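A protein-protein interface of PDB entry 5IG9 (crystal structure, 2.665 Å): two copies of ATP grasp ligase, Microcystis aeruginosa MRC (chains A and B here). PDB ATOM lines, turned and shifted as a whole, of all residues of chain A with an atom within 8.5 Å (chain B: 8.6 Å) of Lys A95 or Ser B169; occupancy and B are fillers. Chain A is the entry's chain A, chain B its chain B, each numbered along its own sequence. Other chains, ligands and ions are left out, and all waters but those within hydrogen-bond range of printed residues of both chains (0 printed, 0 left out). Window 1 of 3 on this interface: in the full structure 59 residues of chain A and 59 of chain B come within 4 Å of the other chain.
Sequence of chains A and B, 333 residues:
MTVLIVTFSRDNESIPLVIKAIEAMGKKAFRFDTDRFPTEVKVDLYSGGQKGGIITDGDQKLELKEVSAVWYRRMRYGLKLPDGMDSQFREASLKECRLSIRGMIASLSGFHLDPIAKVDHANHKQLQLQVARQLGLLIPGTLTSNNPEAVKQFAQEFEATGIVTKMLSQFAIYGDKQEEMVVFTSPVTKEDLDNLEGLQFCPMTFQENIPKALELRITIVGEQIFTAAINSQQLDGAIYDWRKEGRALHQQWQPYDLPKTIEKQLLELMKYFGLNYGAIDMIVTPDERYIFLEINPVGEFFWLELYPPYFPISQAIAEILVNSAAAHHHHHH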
ATOM      1  N   TYR A  77      26.487   4.639  14.071  1.00  0.00           N
ATOM      2  CA  TYR A  77      26.860   5.099  15.404  1.00  0.00           C
ATOM      3  C   TYR A  77      26.749   3.980  16.433  1.00  0.00           C
ATOM      4  O   TYR A  77      25.663   3.442  16.665  1.00  0.00           O
ATOM      5  CB  TYR A  77      25.983   6.277  15.817  1.00  0.00           C
ATOM      6  CG  TYR A  77      25.848   7.348  14.762  1.00  0.00           C
ATOM      7  CD1 TYR A  77      26.890   8.226  14.495  1.00  0.00           C
ATOM      8  CD2 TYR A  77      24.670   7.489  14.041  1.00  0.00           C
ATOM      9  CE1 TYR A  77      26.764   9.208  13.532  1.00  0.00           C
ATOM     10  CE2 TYR A  77      24.535   8.467  13.081  1.00  0.00           C
ATOM     11  CZ  TYR A  77      25.583   9.324  12.831  1.00  0.00           C
ATOM     12  OH  TYR A  77      25.448  10.301  11.873  1.00  0.00           O
ATOM     13  N   GLY A  78      27.881   3.635  17.045  1.00  0.00           N
ATOM     14  CA  GLY A  78      27.893   2.745  18.191  1.00  0.00           C
ATOM     15  C   GLY A  78      27.620   1.285  17.915  1.00  0.00           C
ATOM     16  O   GLY A  78      27.177   0.573  18.823  1.00  0.00           O
ATOM     17  N   LEU A  81      29.224  -1.526  20.116  1.00  0.00           N
ATOM     18  CA  LEU A  81      28.870  -1.705  21.514  1.00  0.00           C
ATOM     19  C   LEU A  81      28.763  -3.197  21.818  1.00  0.00           C
ATOM     20  O   LEU A  81      28.250  -3.958  20.995  1.00  0.00           O
ATOM     21  CB  LEU A  81      27.548  -1.018  21.846  1.00  0.00           C
ATOM     22  CG  LEU A  81      27.621   0.489  22.090  1.00  0.00           C
ATOM     23  CD1 LEU A  81      26.231   1.081  22.274  1.00  0.00           C
ATOM     24  CD2 LEU A  81      28.494   0.781  23.297  1.00  0.00           C
ATOM     25  N   GLN A  88      18.155  -2.792  27.073  1.00  0.00           N
ATOM     26  CA  GLN A  88      17.565  -1.480  27.318  1.00  0.00           C
ATOM     27  C   GLN A  88      18.631  -0.392  27.336  1.00  0.00           C
ATOM     28  O   GLN A  88      18.436   0.685  26.759  1.00  0.00           O
ATOM     29  CB  GLN A  88      16.778  -1.485  28.626  1.00  0.00           C
ATOM     30  CG  GLN A  88      15.454  -2.222  28.544  1.00  0.00           C
ATOM     31  CD  GLN A  88      14.341  -1.494  29.271  1.00  0.00           C
ATOM     32  OE1 GLN A  88      13.790  -0.514  28.766  1.00  0.00           O
ATOM     33  NE2 GLN A  88      14.006  -1.966  30.467  1.00  0.00           N
ATOM     34  N   PHE A  89      19.766  -0.655  27.986  1.00  0.00           N
ATOM     35  CA  PHE A  89      20.849   0.322  27.999  1.00  0.00           C
ATOM     36  C   PHE A  89      21.510   0.444  26.633  1.00  0.00           C
ATOM     37  O   PHE A  89      21.971   1.530  26.263  1.00  0.00           O
ATOM     38  CB  PHE A  89      21.893  -0.050  29.053  1.00  0.00           C
ATOM     39  CG  PHE A  89      21.422   0.118  30.474  1.00  0.00           C
ATOM     40  CD1 PHE A  89      20.250   0.800  30.765  1.00  0.00           C
ATOM     41  CD2 PHE A  89      22.164  -0.402  31.520  1.00  0.00           C
ATOM     42  CE1 PHE A  89      19.828   0.951  32.079  1.00  0.00           C
ATOM     43  CE2 PHE A  89      21.749  -0.251  32.831  1.00  0.00           C
ATOM     44  CZ  PHE A  89      20.579   0.425  33.110  1.00  0.00           C
ATOM     45  N   ARG A  90      21.565  -0.651  25.873  1.00  0.00           N
ATOM     46  CA  ARG A  90      22.220  -0.620  24.569  1.00  0.00           C
ATOM     47  C   ARG A  90      21.436   0.227  23.575  1.00  0.00           C
ATOM     48  O   ARG A  90      22.021   1.017  22.828  1.00  0.00           O
ATOM     49  CB  ARG A  90      22.397  -2.040  24.033  1.00  0.00           C
ATOM     50  CG  ARG A  90      23.481  -2.165  22.977  1.00  0.00           C
ATOM     51  CD  ARG A  90      23.278  -3.402  22.114  1.00  0.00           C
ATOM     52  NE  ARG A  90      24.490  -3.757  21.380  1.00  0.00           N
ATOM     53  CZ  ARG A  90      24.898  -3.155  20.267  1.00  0.00           C
ATOM     54  NH1 ARG A  90      24.195  -2.155  19.752  1.00  0.00           N
ATOM     55  NH2 ARG A  90      26.014  -3.548  19.671  1.00  0.00           N
ATOM     56  N   GLU A  91      20.112   0.068  23.540  1.00  0.00           N
ATOM     57  CA  GLU A  91      19.305   0.865  22.622  1.00  0.00           C
ATOM     58  C   GLU A  91      19.347   2.342  22.996  1.00  0.00           C
ATOM     59  O   GLU A  91      19.389   3.212  22.118  1.00  0.00           O
ATOM     60  CB  GLU A  91      17.864   0.353  22.601  1.00  0.00           C
ATOM     61  CG  GLU A  91      17.705  -1.059  22.051  1.00  0.00           C
ATOM     62  CD  GLU A  91      18.353  -1.239  20.689  1.00  0.00           C
ATOM     63  OE1 GLU A  91      19.513  -1.702  20.634  1.00  0.00           O
ATOM     64  OE2 GLU A  91      17.706  -0.910  19.672  1.00  0.00           O
ATOM     65  N   ALA A  92      19.353   2.641  24.298  1.00  0.00           N
ATOM     66  CA  ALA A  92      19.420   4.028  24.745  1.00  0.00           C
ATOM     67  C   ALA A  92      20.790   4.634  24.464  1.00  0.00           C
ATOM     68  O   ALA A  92      20.896   5.820  24.133  1.00  0.00           O
ATOM     69  CB  ALA A  92      19.091   4.113  26.234  1.00  0.00           C
ATOM     70  N   SER A  93      21.851   3.835  24.599  1.00  0.00           N
ATOM     71  CA  SER A  93      23.192   4.320  24.293  1.00  0.00           C
ATOM     72  C   SER A  93      23.341   4.628  22.809  1.00  0.00           C
ATOM     73  O   SER A  93      23.984   5.617  22.439  1.00  0.00           O
ATOM     74  CB  SER A  93      24.235   3.292  24.734  1.00  0.00           C
ATOM     75  OG  SER A  93      25.545   3.717  24.403  1.00  0.00           O
ATOM     76  N   LEU A  94      22.762   3.789  21.945  1.00  0.00           N
ATOM     77  CA  LEU A  94      22.827   4.044  20.510  1.00  0.00           C
ATOM     78  C   LEU A  94      22.175   5.376  20.161  1.00  0.00           C
ATOM     79  O   LEU A  94      22.720   6.163  19.380  1.00  0.00           O
ATOM     80  CB  LEU A  94      22.156   2.907  19.740  1.00  0.00           C
ATOM     81  CG  LEU A  94      22.863   1.554  19.704  1.00  0.00           C
ATOM     82  CD1 LEU A  94      22.017   0.521  18.973  1.00  0.00           C
ATOM     83  CD2 LEU A  94      24.223   1.687  19.052  1.00  0.00           C
ATOM     84  N   LYS A  95      21.004   5.644  20.736  1.00  0.00           N
ATOM     85  CA  LYS A  95      20.298   6.885  20.440  1.00  0.00           C
ATOM     86  C   LYS A  95      21.054   8.099  20.966  1.00  0.00           C
ATOM     87  O   LYS A  95      21.007   9.169  20.350  1.00  0.00           O
ATOM     88  CB  LYS A  95      18.887   6.826  21.025  1.00  0.00           C
ATOM     89  CG  LYS A  95      17.992   7.987  20.637  1.00  0.00           C
ATOM     90  CD  LYS A  95      16.549   7.704  21.021  1.00  0.00           C
ATOM     91  CE  LYS A  95      15.675   8.932  20.827  1.00  0.00           C
ATOM     92  NZ  LYS A  95      15.742   9.462  19.437  1.00  0.00           N
ATOM     93  N   GLU A  96      21.757   7.954  22.093  1.00  0.00           N
ATOM     94  CA  GLU A  96      22.554   9.062  22.610  1.00  0.00           C
ATOM     95  C   GLU A  96      23.780   9.313  21.742  1.00  0.00           C
ATOM     96  O   GLU A  96      24.136  10.467  21.479  1.00  0.00           O
ATOM     97  CB  GLU A  96      22.969   8.783  24.055  1.00  0.00           C
ATOM     98  CG  GLU A  96      23.731   9.919  24.719  1.00  0.00           C
ATOM     99  CD  GLU A  96      22.837  11.086  25.094  1.00  0.00           C
ATOM    100  OE1 GLU A  96      21.606  10.889  25.188  1.00  0.00           O
ATOM    101  OE2 GLU A  96      23.368  12.198  25.296  1.00  0.00           O
ATOM    102  N   CYS A  97      24.440   8.243  21.292  1.00  0.00           N
ATOM    103  CA  CYS A  97      25.589   8.391  20.403  1.00  0.00           C
ATOM    104  C   CYS A  97      25.185   9.043  19.089  1.00  0.00           C
ATOM    105  O   CYS A  97      25.878   9.935  18.585  1.00  0.00           O
ATOM    106  CB  CYS A  97      26.229   7.029  20.140  1.00  0.00           C
ATOM    107  SG  CYS A  97      26.942   6.245  21.593  1.00  0.00           S
ATOM    108  N   ARG A  98      24.058   8.609  18.520  1.00  0.00           N
ATOM    109  CA  ARG A  98      23.613   9.150  17.240  1.00  0.00           C
ATOM    110  C   ARG A  98      23.318  10.640  17.350  1.00  0.00           C
ATOM    111  O   ARG A  98      23.766  11.436  16.519  1.00  0.00           O
ATOM    112  CB  ARG A  98      22.385   8.381  16.749  1.00  0.00           C
ATOM    113  CG  ARG A  98      21.772   8.928  15.470  1.00  0.00           C
ATOM    114  CD  ARG A  98      20.548   8.124  15.069  1.00  0.00           C
ATOM    115  NE  ARG A  98      19.456   8.991  14.641  1.00  0.00           N
ATOM    116  CZ  ARG A  98      19.232   9.350  13.383  1.00  0.00           C
ATOM    117  NH1 ARG A  98      20.023   8.911  12.411  1.00  0.00           N
ATOM    118  NH2 ARG A  98      18.212  10.146  13.095  1.00  0.00           N
ATOM    119  N   LEU A  99      22.579  11.042  18.386  1.00  0.00           N
ATOM    120  CA  LEU A  99      22.289  12.459  18.582  1.00  0.00           C
ATOM    121  C   LEU A  99      23.555  13.270  18.834  1.00  0.00           C
ATOM    122  O   LEU A  99      23.636  14.435  18.424  1.00  0.00           O
ATOM    123  CB  LEU A  99      21.320  12.643  19.745  1.00  0.00           C
ATOM    124  CG  LEU A  99      19.881  12.207  19.498  1.00  0.00           C
ATOM    125  CD1 LEU A  99      19.074  12.500  20.734  1.00  0.00           C
ATOM    126  CD2 LEU A  99      19.305  12.927  18.293  1.00  0.00           C
ATOM    127  N   SER A 100      24.545  12.680  19.508  1.00  0.00           N
ATOM    128  CA  SER A 100      25.784  13.397  19.800  1.00  0.00           C
ATOM    129  C   SER A 100      26.578  13.674  18.530  1.00  0.00           C
ATOM    130  O   SER A 100      26.994  14.811  18.280  1.00  0.00           O
ATOM    131  CB  SER A 100      26.641  12.599  20.784  1.00  0.00           C
ATOM    132  OG  SER A 100      25.927  12.265  21.958  1.00  0.00           O
ATOM    133  N   ILE A 101      26.818  12.636  17.726  1.00  0.00           N
ATOM    134  CA  ILE A 101      27.646  12.803  16.537  1.00  0.00           C
ATOM    135  C   ILE A 101      26.906  13.597  15.473  1.00  0.00           C
ATOM    136  O   ILE A 101      27.523  14.348  14.711  1.00  0.00           O
ATOM    137  CB  ILE A 101      28.106  11.434  16.004  1.00  0.00           C
ATOM    138  CG1 ILE A 101      28.757  10.625  17.125  1.00  0.00           C
ATOM    139  CG2 ILE A 101      29.092  11.619  14.864  1.00  0.00           C
ATOM    140  CD1 ILE A 101      29.945  11.319  17.769  1.00  0.00           C
ATOM    141  N   ARG A 102      25.583  13.451  15.396  1.00  0.00           N
ATOM    142  CA  ARG A 102      24.804  14.285  14.486  1.00  0.00           C
ATOM    143  C   ARG A 102      24.916  15.755  14.855  1.00  0.00           C
ATOM    144  O   ARG A 102      25.018  16.617  13.975  1.00  0.00           O
ATOM    145  CB  ARG A 102      23.339  13.851  14.490  1.00  0.00           C
ATOM    146  CG  ARG A 102      23.058  12.603  13.683  1.00  0.00           C
ATOM    147  CD  ARG A 102      21.610  12.181  13.825  1.00  0.00           C
ATOM    148  NE  ARG A 102      20.678  13.192  13.330  1.00  0.00           N
ATOM    149  CZ  ARG A 102      20.191  13.219  12.093  1.00  0.00           C
ATOM    150  NH1 ARG A 102      20.552  12.291  11.219  1.00  0.00           N
ATOM    151  NH2 ARG A 102      19.346  14.174  11.730  1.00  0.00           N
ATOM    152  N   ARG B  98       7.169   4.806  10.541  1.00  0.00           N
ATOM    153  CA  ARG B  98       7.713   6.145  10.738  1.00  0.00           C
ATOM    154  C   ARG B  98       8.089   6.784   9.406  1.00  0.00           C
ATOM    155  O   ARG B  98       7.710   7.926   9.125  1.00  0.00           O
ATOM    156  CB  ARG B  98       8.921   6.083  11.673  1.00  0.00           C
ATOM    157  CG  ARG B  98       9.633   7.409  11.866  1.00  0.00           C
ATOM    158  CD  ARG B  98      10.833   7.254  12.783  1.00  0.00           C
ATOM    159  NE  ARG B  98      11.564   8.506  12.947  1.00  0.00           N
ATOM    160  CZ  ARG B  98      12.583   8.878  12.181  1.00  0.00           C
ATOM    161  NH1 ARG B  98      12.995   8.097  11.193  1.00  0.00           N
ATOM    162  NH2 ARG B  98      13.193  10.034  12.403  1.00  0.00           N
ATOM    163  N   ASN B 123      16.680  20.177  16.232  1.00  0.00           N
ATOM    164  CA  ASN B 123      16.814  19.154  17.265  1.00  0.00           C
ATOM    165  C   ASN B 123      18.247  18.978  17.750  1.00  0.00           C
ATOM    166  O   ASN B 123      18.452  18.344  18.790  1.00  0.00           O
ATOM    167  CB  ASN B 123      16.284  17.811  16.763  1.00  0.00           C
ATOM    168  CG  ASN B 123      14.775  17.702  16.868  1.00  0.00           C
ATOM    169  OD1 ASN B 123      14.143  18.403  17.655  1.00  0.00           O
ATOM    170  ND2 ASN B 123      14.189  16.813  16.070  1.00  0.00           N
ATOM    171  N   LYS B 125      20.904  19.978  19.801  1.00  0.00           N
ATOM    172  CA  LYS B 125      21.048  20.899  20.922  1.00  0.00           C
ATOM    173  C   LYS B 125      22.409  21.583  20.921  1.00  0.00           C
ATOM    174  O   LYS B 125      22.530  22.721  21.389  1.00  0.00           O
ATOM    175  CB  LYS B 125      20.814  20.163  22.241  1.00  0.00           C
ATOM    176  CG  LYS B 125      19.399  19.622  22.398  1.00  0.00           C
ATOM    177  CD  LYS B 125      19.237  18.850  23.700  1.00  0.00           C
ATOM    178  CE  LYS B 125      17.794  18.402  23.901  1.00  0.00           C
ATOM    179  NZ  LYS B 125      17.602  17.621  25.156  1.00  0.00           N
ATOM    180  N   LYS B 166      23.435  15.470  31.786  1.00  0.00           N
ATOM    181  CA  LYS B 166      22.130  15.241  31.189  1.00  0.00           C
ATOM    182  C   LYS B 166      22.305  14.436  29.910  1.00  0.00           C
ATOM    183  O   LYS B 166      23.388  14.393  29.321  1.00  0.00           O
ATOM    184  CB  LYS B 166      21.400  16.554  30.908  1.00  0.00           C
ATOM    185  CG  LYS B 166      22.045  17.407  29.826  1.00  0.00           C
ATOM    186  CD  LYS B 166      21.345  18.755  29.718  1.00  0.00           C
ATOM    187  CE  LYS B 166      21.982  19.651  28.666  1.00  0.00           C
ATOM    188  NZ  LYS B 166      21.703  19.193  27.277  1.00  0.00           N
ATOM    189  N   MET B 167      21.218  13.796  29.491  1.00  0.00           N
ATOM    190  CA  MET B 167      21.187  13.022  28.260  1.00  0.00           C
ATOM    191  C   MET B 167      20.584  13.866  27.146  1.00  0.00           C
ATOM    192  O   MET B 167      19.609  14.593  27.364  1.00  0.00           O
ATOM    193  CB  MET B 167      20.377  11.735  28.441  1.00  0.00           C
ATOM    194  CG  MET B 167      20.999  10.729  29.398  1.00  0.00           C
ATOM    195  SD  MET B 167      22.546  10.021  28.797  1.00  0.00           S
ATOM    196  CE  MET B 167      21.948   8.729  27.707  1.00  0.00           C
ATOM    197  N   LEU B 168      21.180  13.782  25.955  1.00  0.00           N
ATOM    198  CA  LEU B 168      20.609  14.480  24.809  1.00  0.00           C
ATOM    199  C   LEU B 168      19.309  13.835  24.357  1.00  0.00           C
ATOM    200  O   LEU B 168      18.427  14.521  23.829  1.00  0.00           O
ATOM    201  CB  LEU B 168      21.608  14.509  23.655  1.00  0.00           C
ATOM    202  CG  LEU B 168      22.839  15.399  23.821  1.00  0.00           C
ATOM    203  CD1 LEU B 168      23.759  15.229  22.628  1.00  0.00           C
ATOM    204  CD2 LEU B 168      22.430  16.854  23.989  1.00  0.00           C
ATOM    205  N   SER B 169      19.166  12.533  24.569  1.00  0.00           N
ATOM    206  CA  SER B 169      18.021  11.783  24.081  1.00  0.00           C
ATOM    207  C   SER B 169      16.924  11.690  25.137  1.00  0.00           C
ATOM    208  O   SER B 169      17.141  11.933  26.327  1.00  0.00           O
ATOM    209  CB  SER B 169      18.450  10.380  23.650  1.00  0.00           C
ATOM    210  OG  SER B 169      19.126   9.710  24.699  1.00  0.00           O
ATOM    211  N   GLN B 170      15.728  11.341  24.673  1.00  0.00           N
ATOM    212  CA  GLN B 170      14.587  11.052  25.530  1.00  0.00           C
ATOM    213  C   GLN B 170      14.332   9.555  25.513  1.00  0.00           C
ATOM    214  O   GLN B 170      14.239   8.953  24.439  1.00  0.00           O
ATOM    215  CB  GLN B 170      13.338  11.801  25.066  1.00  0.00           C
ATOM    216  CG  GLN B 170      13.488  13.306  25.026  1.00  0.00           C
ATOM    217  CD  GLN B 170      12.167  14.017  24.809  1.00  0.00           C
ATOM    218  OE1 GLN B 170      11.101  13.399  24.837  1.00  0.00           O
ATOM    219  NE2 GLN B 170      12.231  15.326  24.592  1.00  0.00           N
ATOM    220  N   PHE B 171      14.219   8.960  26.694  1.00  0.00           N
ATOM    221  CA  PHE B 171      13.969   7.527  26.807  1.00  0.00           C
ATOM    222  C   PHE B 171      13.495   7.237  28.226  1.00  0.00           C
ATOM    223  O   PHE B 171      13.324   8.144  29.047  1.00  0.00           O
ATOM    224  CB  PHE B 171      15.216   6.713  26.452  1.00  0.00           C
ATOM    225  CG  PHE B 171      16.397   7.006  27.328  1.00  0.00           C
ATOM    226  CD1 PHE B 171      16.585   6.316  28.514  1.00  0.00           C
ATOM    227  CD2 PHE B 171      17.321   7.973  26.969  1.00  0.00           C
ATOM    228  CE1 PHE B 171      17.667   6.584  29.325  1.00  0.00           C
ATOM    229  CE2 PHE B 171      18.405   8.246  27.776  1.00  0.00           C
ATOM    230  CZ  PHE B 171      18.580   7.549  28.955  1.00  0.00           C
ATOM    231  N   ALA B 172      13.285   5.952  28.504  1.00  0.00           N
ATOM    232  CA  ALA B 172      12.918   5.496  29.837  1.00  0.00           C
ATOM    233  C   ALA B 172      13.292   4.027  29.962  1.00  0.00           C
ATOM    234  O   ALA B 172      12.995   3.233  29.066  1.00  0.00           O
ATOM    235  CB  ALA B 172      11.422   5.696  30.105  1.00  0.00           C
ATOM    236  N   VAL B 182      14.056   7.378  34.595  1.00  0.00           N
ATOM    237  CA  VAL B 182      14.355   8.502  33.714  1.00  0.00           C
ATOM    238  C   VAL B 182      15.569   9.239  34.266  1.00  0.00           C
ATOM    239  O   VAL B 182      15.718   9.391  35.482  1.00  0.00           O
ATOM    240  CB  VAL B 182      13.128   9.432  33.574  1.00  0.00           C
ATOM    241  CG1 VAL B 182      13.548  10.879  33.360  1.00  0.00           C
ATOM    242  CG2 VAL B 182      12.240   8.963  32.431  1.00  0.00           C
ATOM    243  N   VAL B 183      16.447   9.680  33.365  1.00  0.00           N
ATOM    244  CA  VAL B 183      17.635  10.446  33.733  1.00  0.00           C
ATOM    245  C   VAL B 183      17.273  11.926  33.647  1.00  0.00           C
ATOM    246  O   VAL B 183      17.249  12.511  32.563  1.00  0.00           O
ATOM    247  CB  VAL B 183      18.831  10.111  32.839  1.00  0.00           C
ATOM    248  CG1 VAL B 183      20.016  11.016  33.175  1.00  0.00           C
ATOM    249  CG2 VAL B 183      19.223   8.654  32.986  1.00  0.00           C
ATOM    250  N   PHE B 184      16.988  12.532  34.797  1.00  0.00           N
ATOM    251  CA  PHE B 184      16.824  13.974  34.865  1.00  0.00           C
ATOM    252  C   PHE B 184      18.186  14.658  34.852  1.00  0.00           C
ATOM    253  O   PHE B 184      19.237  14.013  34.873  1.00  0.00           O
ATOM    254  CB  PHE B 184      16.061  14.378  36.127  1.00  0.00           C
ATOM    255  CG  PHE B 184      14.619  13.975  36.124  1.00  0.00           C
ATOM    256  CD1 PHE B 184      13.723  14.566  35.250  1.00  0.00           C
ATOM    257  CD2 PHE B 184      14.155  13.022  37.012  1.00  0.00           C
ATOM    258  CE1 PHE B 184      12.391  14.199  35.253  1.00  0.00           C
ATOM    259  CE2 PHE B 184      12.825  12.650  37.021  1.00  0.00           C
ATOM    260  CZ  PHE B 184      11.941  13.240  36.140  1.00  0.00           C
ATOM    261  N   PHE B 201      30.759   3.305  27.053  1.00  0.00           N
ATOM    262  CA  PHE B 201      29.567   2.616  26.592  1.00  0.00           C
ATOM    263  C   PHE B 201      28.430   3.562  26.242  1.00  0.00           C
ATOM    264  O   PHE B 201      27.493   3.149  25.549  1.00  0.00           O
ATOM    265  CB  PHE B 201      29.096   1.615  27.658  1.00  0.00           C
ATOM    266  CG  PHE B 201      30.146   0.614  28.050  1.00  0.00           C
ATOM    267  CD1 PHE B 201      30.843  -0.090  27.083  1.00  0.00           C
ATOM    268  CD2 PHE B 201      30.450   0.390  29.382  1.00  0.00           C
ATOM    269  CE1 PHE B 201      31.813  -1.007  27.437  1.00  0.00           C
ATOM    270  CE2 PHE B 201      31.422  -0.526  29.744  1.00  0.00           C
ATOM    271  CZ  PHE B 201      32.104  -1.225  28.768  1.00  0.00           C
ATOM    272  N   CYS B 202      28.488   4.812  26.695  1.00  0.00           N
ATOM    273  CA  CYS B 202      27.501   5.827  26.359  1.00  0.00           C
ATOM    274  C   CYS B 202      28.010   7.191  26.805  1.00  0.00           C
ATOM    275  O   CYS B 202      28.354   7.373  27.980  1.00  0.00           O
ATOM    276  CB  CYS B 202      26.150   5.524  27.012  1.00  0.00           C
ATOM    277  SG  CYS B 202      24.835   6.705  26.616  1.00  0.00           S
ATOM    278  N   PRO B 203      28.077   8.168  25.908  1.00  0.00           N
ATOM    279  CA  PRO B 203      28.491   9.512  26.312  1.00  0.00           C
ATOM    280  C   PRO B 203      27.378  10.213  27.075  1.00  0.00           C
ATOM    281  O   PRO B 203      26.226   9.778  27.104  1.00  0.00           O
ATOM    282  CB  PRO B 203      28.779  10.202  24.979  1.00  0.00           C
ATOM    283  CG  PRO B 203      27.839   9.549  24.040  1.00  0.00           C
ATOM    284  CD  PRO B 203      27.749   8.106  24.474  1.00  0.00           C
ATOM    285  N   MET B 204      27.748  11.319  27.714  1.00  0.00           N
ATOM    286  CA  MET B 204      26.786  12.182  28.381  1.00  0.00           C
ATOM    287  C   MET B 204      27.143  13.629  28.087  1.00  0.00           C
ATOM    288  O   MET B 204      28.231  13.938  27.595  1.00  0.00           O
ATOM    289  CB  MET B 204      26.744  11.937  29.899  1.00  0.00           C
ATOM    290  CG  MET B 204      26.245  10.557  30.301  1.00  0.00           C
ATOM    291  SD  MET B 204      25.559  10.507  31.969  1.00  0.00           S
ATOM    292  CE  MET B 204      24.080  11.498  31.765  1.00  0.00           C
ATOM    293  N   THR B 205      26.209  14.521  28.392  1.00  0.00           N
ATOM    294  CA  THR B 205      26.383  15.952  28.183  1.00  0.00           C
ATOM    295  C   THR B 205      26.479  16.633  29.542  1.00  0.00           C
ATOM    296  O   THR B 205      25.519  16.613  30.320  1.00  0.00           O
ATOM    297  CB  THR B 205      25.229  16.528  27.362  1.00  0.00           C
ATOM    298  OG1 THR B 205      25.154  15.844  26.106  1.00  0.00           O
ATOM    299  CG2 THR B 205      25.446  18.004  27.105  1.00  0.00           C
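SG of Cys B202 lies close to OG of Ser A93. The backbone NH of Leu B168 is in hydrogen-bond range of the side-chain carboxylate of Glu A96 (2.8 Å). OE1 of Glu A96 is in hydrogen-bond range of OG of Ser B169, at 2.8 Å. The side-chain hydroxyl (OG) of Ser A93 lies close to the backbone carbonyl oxygen (O) of Phe B201, at 2.3 Å.
NH2 of Arg A90 sits at hydrogen-bond distance from O of Leu A81, at 2.6 Å. The backbone carbonyl oxygen of Ser A93 is in hydrogen-bond range of the side-chain sulfur of Cys A97 (3.1 Å). The backbone carbonyl oxygen (O) of Glu A96 is in hydrogen-bond range of the side-chain hydroxyl (OG) of Ser A100, at 2.6 Å. The backbone carbonyl oxygen of Leu B168 sits at hydrogen-bond distance from the side-chain amino group of Lys B125 (3.5 Å).
Among the printed residues, merely in contact across the chains: Leu A81 with Phe B201, Gln A88 with Ala B172, Lys A95 with Ser B169, Lys A95 with Gln B170, Glu A96 with Met B167, Glu A96 with Cys B202, Glu A96 with Pro B203, Cys A97 with Pro B203, Leu A99 with Leu B168, Leu A99 with Ser B169, Ser A100 with Leu B168 and Ser A100 with Pro B203.
Of chain B, only Ser B169 and Gln B170 come within 4 Å of Lys A95. Of chain A, only Lys A95 (3.9 Å), Glu A96 (2.8 Å) and Leu A99 (3.6 Å) come within 4 Å of Ser B169. Printed residues of chain A within 4 Å of Pro B203: Glu A96 (3.5 Å), Cys A97 (3.5 Å) and Ser A100 (3.9 Å). Printed residues of chain A within 4 Å of Ala B172: Gln A88. Of the printed residues of chain B, Ser A100 touches Leu B168 and Pro B203. Of the printed residues of chain A, Gln B170 touches Lys A95. Printed residues of chain B within 4 Å of Gln A88: Ala B172. Gly A78 touches none of the printed residues of chain B. Ile A101 touches none of the printed residues of chain B. The nearest residue of chain A that does not touch Ser B169 is Ala A92 (4.3 Å).
Of the 18 printed residues of chain A, 8 touch a printed residue of chain B. Of the 18 printed residues of chain B, 8 touch a printed residue of chain A. Printed residues of chain B that touch a printed residue of chain A: Met B167, Leu B168, Ser B169, Gln B170, Ala B172, Phe B201, Cys B202 and Pro B203. Hydrophobic or aromatic side chains of chain B that line the printed part of chain A: Met B167, Leu B168 and Pro B203. Among the printed residues, no Asp or Glu carboxylate lies within 4 Å of a Lys or Arg side-chain nitrogen of the other chain.
Position printed for both chains: 98. Of the 16 pairs that touch across the chains among the printed residues, none has its exchanged pair printed and touching as well.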
